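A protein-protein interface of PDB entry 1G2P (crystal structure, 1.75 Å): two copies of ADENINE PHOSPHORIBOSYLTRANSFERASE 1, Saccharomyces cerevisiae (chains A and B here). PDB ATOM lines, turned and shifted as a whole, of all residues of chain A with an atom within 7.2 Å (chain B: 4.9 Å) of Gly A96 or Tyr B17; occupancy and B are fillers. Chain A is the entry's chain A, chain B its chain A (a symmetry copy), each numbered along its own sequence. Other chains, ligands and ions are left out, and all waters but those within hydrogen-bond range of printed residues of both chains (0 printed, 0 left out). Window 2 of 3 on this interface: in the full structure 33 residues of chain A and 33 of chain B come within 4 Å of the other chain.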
ATOM      1  N   LEU A  94      15.687 -16.081 -14.610  1.00  0.00           N
ATOM      2  CA  LEU A  94      15.105 -14.769 -14.875  1.00  0.00           C
ATOM      3  C   LEU A  94      16.052 -13.788 -15.554  1.00  0.00           C
ATOM      4  O   LEU A  94      17.216 -13.672 -15.174  1.00  0.00           O
ATOM      5  CB  LEU A  94      14.626 -14.139 -13.572  1.00  0.00           C
ATOM      6  CG  LEU A  94      13.458 -14.840 -12.872  1.00  0.00           C
ATOM      7  CD1 LEU A  94      13.389 -14.374 -11.428  1.00  0.00           C
ATOM      8  CD2 LEU A  94      12.159 -14.535 -13.619  1.00  0.00           C
ATOM      9  N   PRO A  95      15.558 -13.058 -16.567  1.00  0.00           N
ATOM     10  CA  PRO A  95      16.390 -12.077 -17.270  1.00  0.00           C
ATOM     11  C   PRO A  95      16.310 -10.750 -16.520  1.00  0.00           C
ATOM     12  O   PRO A  95      15.359 -10.517 -15.766  1.00  0.00           O
ATOM     13  CB  PRO A  95      15.720 -11.981 -18.633  1.00  0.00           C
ATOM     14  CG  PRO A  95      14.276 -12.052 -18.261  1.00  0.00           C
ATOM     15  CD  PRO A  95      14.255 -13.208 -17.239  1.00  0.00           C
ATOM     16  N   GLY A  96      17.296  -9.883 -16.730  1.00  0.00           N
ATOM     17  CA  GLY A  96      17.288  -8.588 -16.079  1.00  0.00           C
ATOM     18  C   GLY A  96      17.836  -8.603 -14.667  1.00  0.00           C
ATOM     19  O   GLY A  96      18.280  -9.631 -14.169  1.00  0.00           O
ATOM     20  N   GLU A  97      17.792  -7.442 -14.025  1.00  0.00           N
ATOM     21  CA  GLU A  97      18.276  -7.271 -12.661  1.00  0.00           C
ATOM     22  C   GLU A  97      17.387  -8.006 -11.660  1.00  0.00           C
ATOM     23  O   GLU A  97      16.175  -7.761 -11.602  1.00  0.00           O
ATOM     24  CB  GLU A  97      18.292  -5.787 -12.305  1.00  0.00           C
ATOM     25  CG  GLU A  97      19.270  -4.953 -13.104  1.00  0.00           C
ATOM     26  CD  GLU A  97      20.711  -5.293 -12.790  1.00  0.00           C
ATOM     27  OE1 GLU A  97      21.220  -6.296 -13.332  1.00  0.00           O
ATOM     28  OE2 GLU A  97      21.331  -4.562 -11.987  1.00  0.00           O
ATOM     29  N   CYS A  98      18.002  -8.877 -10.863  1.00  0.00           N
ATOM     30  CA  CYS A  98      17.289  -9.660  -9.854  1.00  0.00           C
ATOM     31  C   CYS A  98      17.860  -9.581  -8.443  1.00  0.00           C
ATOM     32  O   CYS A  98      19.061  -9.389  -8.254  1.00  0.00           O
ATOM     33  CB  CYS A  98      17.296 -11.147 -10.225  1.00  0.00           C
ATOM     34  SG  CYS A  98      16.506 -11.565 -11.759  1.00  0.00           S
ATOM     35  N   PHE A  99      16.985  -9.726  -7.453  1.00  0.00           N
ATOM     36  CA  PHE A  99      17.429  -9.797  -6.073  1.00  0.00           C
ATOM     37  C   PHE A  99      17.692 -11.291  -5.917  1.00  0.00           C
ATOM     38  O   PHE A  99      17.101 -12.101  -6.639  1.00  0.00           O
ATOM     39  CB  PHE A  99      16.336  -9.350  -5.107  1.00  0.00           C
ATOM     40  CG  PHE A  99      16.222  -7.861  -4.984  1.00  0.00           C
ATOM     41  CD1 PHE A  99      15.003  -7.226  -5.174  1.00  0.00           C
ATOM     42  CD2 PHE A  99      17.344  -7.090  -4.692  1.00  0.00           C
ATOM     43  CE1 PHE A  99      14.897  -5.851  -5.079  1.00  0.00           C
ATOM     44  CE2 PHE A  99      17.250  -5.707  -4.592  1.00  0.00           C
ATOM     45  CZ  PHE A  99      16.027  -5.084  -4.784  1.00  0.00           C
ATOM     46  N   GLU A 113      15.786 -16.195  -7.136  1.00  0.00           N
ATOM     47  CA  GLU A 113      15.792 -14.816  -7.589  1.00  0.00           C
ATOM     48  C   GLU A 113      14.377 -14.329  -7.864  1.00  0.00           C
ATOM     49  O   GLU A 113      13.451 -15.133  -8.029  1.00  0.00           O
ATOM     50  CB  GLU A 113      16.597 -14.680  -8.892  1.00  0.00           C
ATOM     51  CG  GLU A 113      18.096 -15.003  -8.787  1.00  0.00           C
ATOM     52  CD  GLU A 113      18.836 -14.805 -10.108  1.00  0.00           C
ATOM     53  OE1 GLU A 113      18.514 -15.503 -11.095  1.00  0.00           O
ATOM     54  OE2 GLU A 113      19.745 -13.950 -10.159  1.00  0.00           O
ATOM     55  N   ILE A 114      14.237 -13.005  -7.901  1.00  0.00           N
ATOM     56  CA  ILE A 114      12.987 -12.342  -8.242  1.00  0.00           C
ATOM     57  C   ILE A 114      13.455 -11.082  -8.985  1.00  0.00           C
ATOM     58  O   ILE A 114      14.499 -10.518  -8.646  1.00  0.00           O
ATOM     59  CB  ILE A 114      12.139 -11.994  -6.985  1.00  0.00           C
ATOM     60  CG1 ILE A 114      10.686 -11.726  -7.406  1.00  0.00           C
ATOM     61  CG2 ILE A 114      12.706 -10.768  -6.260  1.00  0.00           C
ATOM     62  CD1 ILE A 114       9.686 -11.805  -6.248  1.00  0.00           C
ATOM     63  N   GLN A 115      12.727 -10.669 -10.019  1.00  0.00           N
ATOM     64  CA  GLN A 115      13.115  -9.487 -10.781  1.00  0.00           C
ATOM     65  C   GLN A 115      12.908  -8.225  -9.936  1.00  0.00           C
ATOM     66  O   GLN A 115      11.843  -8.019  -9.365  1.00  0.00           O
ATOM     67  CB  GLN A 115      12.302  -9.404 -12.075  1.00  0.00           C
ATOM     68  CG  GLN A 115      12.537 -10.576 -13.034  1.00  0.00           C
ATOM     69  CD  GLN A 115      11.583 -10.560 -14.215  1.00  0.00           C
ATOM     70  OE1 GLN A 115      10.370 -10.472 -14.041  1.00  0.00           O
ATOM     71  NE2 GLN A 115      12.128 -10.652 -15.423  1.00  0.00           N
ATOM     72  N   LYS A 116      13.935  -7.383  -9.866  1.00  0.00           N
ATOM     73  CA  LYS A 116      13.874  -6.157  -9.070  1.00  0.00           C
ATOM     74  C   LYS A 116      12.738  -5.217  -9.445  1.00  0.00           C
ATOM     75  O   LYS A 116      12.159  -4.562  -8.577  1.00  0.00           O
ATOM     76  CB  LYS A 116      15.204  -5.389  -9.171  1.00  0.00           C
ATOM     77  CG  LYS A 116      16.407  -6.095  -8.533  1.00  0.00           C
ATOM     78  CD  LYS A 116      17.613  -5.150  -8.486  1.00  0.00           C
ATOM     79  CE  LYS A 116      18.800  -5.787  -7.786  1.00  0.00           C
ATOM     80  NZ  LYS A 116      19.951  -4.838  -7.663  1.00  0.00           N
ATOM     81  N   ASN A 117      12.404  -5.149 -10.727  1.00  0.00           N
ATOM     82  CA  ASN A 117      11.350  -4.235 -11.158  1.00  0.00           C
ATOM     83  C   ASN A 117       9.946  -4.838 -11.169  1.00  0.00           C
ATOM     84  O   ASN A 117       8.981  -4.168 -11.539  1.00  0.00           O
ATOM     85  CB  ASN A 117      11.676  -3.691 -12.556  1.00  0.00           C
ATOM     86  CG  ASN A 117      11.406  -4.704 -13.660  1.00  0.00           C
ATOM     87  OD1 ASN A 117      11.849  -5.855 -13.591  1.00  0.00           O
ATOM     88  ND2 ASN A 117      10.680  -4.275 -14.696  1.00  0.00           N
ATOM     89  N   HIS B  15       9.512  -7.581 -22.753  1.00  0.00           N
ATOM     90  CA  HIS B  15      10.773  -6.889 -22.510  1.00  0.00           C
ATOM     91  C   HIS B  15      11.846  -7.723 -23.200  1.00  0.00           C
ATOM     92  O   HIS B  15      11.864  -8.943 -23.054  1.00  0.00           O
ATOM     93  CB  HIS B  15      11.078  -6.816 -21.006  1.00  0.00           C
ATOM     94  CG  HIS B  15      10.243  -5.822 -20.260  1.00  0.00           C
ATOM     95  ND1 HIS B  15      10.241  -5.738 -18.883  1.00  0.00           N
ATOM     96  CD2 HIS B  15       9.393  -4.859 -20.693  1.00  0.00           C
ATOM     97  CE1 HIS B  15       9.428  -4.769 -18.500  1.00  0.00           C
ATOM     98  NE2 HIS B  15       8.902  -4.219 -19.580  1.00  0.00           N
ATOM     99  N   GLN B  16      12.729  -7.085 -23.965  1.00  0.00           N
ATOM    100  CA  GLN B  16      13.794  -7.827 -24.645  1.00  0.00           C
ATOM    101  C   GLN B  16      15.116  -7.726 -23.892  1.00  0.00           C
ATOM    102  O   GLN B  16      15.438  -6.684 -23.325  1.00  0.00           O
ATOM    103  CB  GLN B  16      13.987  -7.317 -26.080  1.00  0.00           C
ATOM    104  CG  GLN B  16      12.920  -7.785 -27.066  1.00  0.00           C
ATOM    105  CD  GLN B  16      13.175  -7.318 -28.498  1.00  0.00           C
ATOM    106  OE1 GLN B  16      14.163  -7.706 -29.130  1.00  0.00           O
ATOM    107  NE2 GLN B  16      12.283  -6.478 -29.013  1.00  0.00           N
ATOM    108  N   TYR B  17      15.868  -8.820 -23.879  1.00  0.00           N
ATOM    109  CA  TYR B  17      17.159  -8.852 -23.214  1.00  0.00           C
ATOM    110  C   TYR B  17      18.194  -9.479 -24.130  1.00  0.00           C
ATOM    111  O   TYR B  17      18.170 -10.688 -24.388  1.00  0.00           O
ATOM    112  CB  TYR B  17      17.092  -9.645 -21.906  1.00  0.00           C
ATOM    113  CG  TYR B  17      16.228  -9.007 -20.850  1.00  0.00           C
ATOM    114  CD1 TYR B  17      14.866  -9.291 -20.772  1.00  0.00           C
ATOM    115  CD2 TYR B  17      16.771  -8.113 -19.928  1.00  0.00           C
ATOM    116  CE1 TYR B  17      14.068  -8.704 -19.802  1.00  0.00           C
ATOM    117  CE2 TYR B  17      15.984  -7.522 -18.961  1.00  0.00           C
ATOM    118  CZ  TYR B  17      14.634  -7.821 -18.901  1.00  0.00           C
ATOM    119  OH  TYR B  17      13.852  -7.244 -17.935  1.00  0.00           O
ATOM    120  N   PRO B  18      19.120  -8.657 -24.646  1.00  0.00           N
ATOM    121  CA  PRO B  18      20.159  -9.172 -25.539  1.00  0.00           C
ATOM    122  C   PRO B  18      21.146 -10.076 -24.811  1.00  0.00           C
ATOM    123  O   PRO B  18      21.524  -9.814 -23.669  1.00  0.00           O
ATOM    124  CB  PRO B  18      20.811  -7.899 -26.074  1.00  0.00           C
ATOM    125  CG  PRO B  18      20.678  -6.950 -24.916  1.00  0.00           C
ATOM    126  CD  PRO B  18      19.259  -7.201 -24.453  1.00  0.00           C
ATOM    127  N   ASN B  19      21.540 -11.152 -25.483  1.00  0.00           N
ATOM    128  CA  ASN B  19      22.494 -12.110 -24.942  1.00  0.00           C
ATOM    129  C   ASN B  19      22.156 -12.590 -23.532  1.00  0.00           C
ATOM    130  O   ASN B  19      23.062 -12.849 -22.740  1.00  0.00           O
ATOM    131  CB  ASN B  19      23.895 -11.487 -24.936  1.00  0.00           C
ATOM    132  CG  ASN B  19      24.214 -10.751 -26.225  1.00  0.00           C
ATOM    133  OD1 ASN B  19      24.259 -11.348 -27.302  1.00  0.00           O
ATOM    134  ND2 ASN B  19      24.432  -9.446 -26.118  1.00  0.00           N
ATOM    135  N   PHE B  20      20.873 -12.721 -23.201  1.00  0.00           N
ATOM    136  CA  PHE B  20      20.558 -13.175 -21.853  1.00  0.00           C
ATOM    137  C   PHE B  20      20.891 -14.638 -21.625  1.00  0.00           C
ATOM    138  O   PHE B  20      21.831 -14.951 -20.888  1.00  0.00           O
ATOM    139  CB  PHE B  20      19.094 -12.962 -21.470  1.00  0.00           C
ATOM    140  CG  PHE B  20      18.708 -13.711 -20.221  1.00  0.00           C
ATOM    141  CD1 PHE B  20      19.397 -13.495 -19.028  1.00  0.00           C
ATOM    142  CD2 PHE B  20      17.718 -14.689 -20.252  1.00  0.00           C
ATOM    143  CE1 PHE B  20      19.109 -14.244 -17.885  1.00  0.00           C
ATOM    144  CE2 PHE B  20      17.421 -15.444 -19.114  1.00  0.00           C
ATOM    145  CZ  PHE B  20      18.120 -15.219 -17.930  1.00  0.00           C
ATOM    146  N   ILE B  25      22.134 -15.061 -27.940  1.00  0.00           N
ATOM    147  CA  ILE B  25      20.744 -15.395 -27.657  1.00  0.00           C
ATOM    148  C   ILE B  25      19.923 -14.207 -27.160  1.00  0.00           C
ATOM    149  O   ILE B  25      20.117 -13.737 -26.039  1.00  0.00           O
ATOM    150  CB  ILE B  25      20.686 -16.530 -26.636  1.00  0.00           C
ATOM    151  N   LEU B  26      19.016 -13.716 -27.999  1.00  0.00           N
ATOM    152  CA  LEU B  26      18.151 -12.603 -27.611  1.00  0.00           C
ATOM    153  C   LEU B  26      16.961 -13.216 -26.871  1.00  0.00           C
ATOM    154  O   LEU B  26      16.315 -14.135 -27.381  1.00  0.00           O
ATOM    155  CB  LEU B  26      17.651 -11.835 -28.841  1.00  0.00           C
ATOM    156  CG  LEU B  26      16.636 -10.721 -28.542  1.00  0.00           C
ATOM    157  CD1 LEU B  26      17.255  -9.702 -27.597  1.00  0.00           C
ATOM    158  CD2 LEU B  26      16.196 -10.046 -29.831  1.00  0.00           C
ATOM    159  N   PHE B  27      16.676 -12.716 -25.673  1.00  0.00           N
ATOM    160  CA  PHE B  27      15.572 -13.256 -24.886  1.00  0.00           C
ATOM    161  C   PHE B  27      14.314 -12.397 -24.887  1.00  0.00           C
ATOM    162  O   PHE B  27      14.382 -11.174 -24.769  1.00  0.00           O
ATOM    163  CB  PHE B  27      16.015 -13.473 -23.441  1.00  0.00           C
ATOM    164  CG  PHE B  27      15.036 -14.262 -22.629  1.00  0.00           C
ATOM    165  CD1 PHE B  27      14.833 -15.614 -22.888  1.00  0.00           C
ATOM    166  CD2 PHE B  27      14.298 -13.655 -21.619  1.00  0.00           C
ATOM    167  CE1 PHE B  27      13.906 -16.352 -22.151  1.00  0.00           C
ATOM    168  CE2 PHE B  27      13.370 -14.383 -20.879  1.00  0.00           C
ATOM    169  CZ  PHE B  27      13.174 -15.734 -21.144  1.00  0.00           C
ATOM    170  N   ASP B  29      11.087 -11.765 -22.782  1.00  0.00           N
ATOM    171  CA  ASP B  29      10.478 -11.993 -21.473  1.00  0.00           C
ATOM    172  C   ASP B  29       9.001 -11.628 -21.432  1.00  0.00           C
ATOM    173  O   ASP B  29       8.650 -10.453 -21.504  1.00  0.00           O
ATOM    174  CB  ASP B  29      11.224 -11.186 -20.409  1.00  0.00           C
ATOM    175  CG  ASP B  29      10.600 -11.325 -19.033  1.00  0.00           C
ATOM    176  OD1 ASP B  29       9.863 -12.315 -18.827  1.00  0.00           O
ATOM    177  OD2 ASP B  29      10.853 -10.460 -18.164  1.00  0.00           O
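Of the printed residues of chain A, Tyr B17 touches Pro A95 (3.5 Å) and Gly A96 (3.3 Å).
Printed residues of chain A within 4 Å of Phe B27: Pro A95.
Printed residues of chain A within 4 Å of Phe B20: Leu A94 and Pro A95.
Of the printed residues of chain A, Asp B29 touches Pro A95 (3.8 Å) and Gln A115 (3.0 Å).
Printed residues of chain B within 4 Å of Pro A95: Tyr B17, Phe B20, Phe B27 and Asp B29.
Asn A117 touches none of the printed residues of chain B.
The nearest residue of chain A that does not touch Tyr B17 is Gln A115 (4.6 Å).
The side-chain amide nitrogen of Gln A115 lies within hydrogen-bond range of the side-chain carboxylate of Asp B29 (3.0 Å).
No position is printed for both chains.
Of the 7 pairs that touch across the chains among the printed residues, none has its exchanged pair printed and touching as well.
Among the printed residues, pairs that only touch across the chains: Leu A94 with Phe B20 (3.3 Å), Gly A96 with Tyr B17 (3.3 Å), Pro A95 with Phe B20 (3.5 Å), Pro A95 with Tyr B17 (3.5 Å), Pro A95 with Phe B27 (3.6 Å) and Pro A95 with Asp B29 (3.8 Å).
NE2 of Gln A115 is in hydrogen-bond range of O of Pro A95, 3.3 Å away.
The backbone carbonyl oxygen (O) of Gly A96 sits at hydrogen-bond distance from the side-chain sulfur (SG) of Cys A98 (3.6 Å).
The backbone NH (N) of Asp B29 sits at hydrogen-bond distance from the backbone carbonyl oxygen (O) of His B15, at 2.9 Å.
The backbone carbonyl oxygen of Tyr B17 lies within hydrogen-bond range of the backbone NH of Phe B27 (2.8 Å).
N of Phe B20 is in hydrogen-bond range of O of Ile B25.
Hydrophobic or aromatic side chains of chain A that line the printed part of chain B: Pro A95.
Of the 10 printed residues of chain B, 4 touch a printed residue of chain A.
Hydrophobic or aromatic side chains of chain B that line the printed part of chain A: Tyr B17, Phe B20 and Phe B27.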
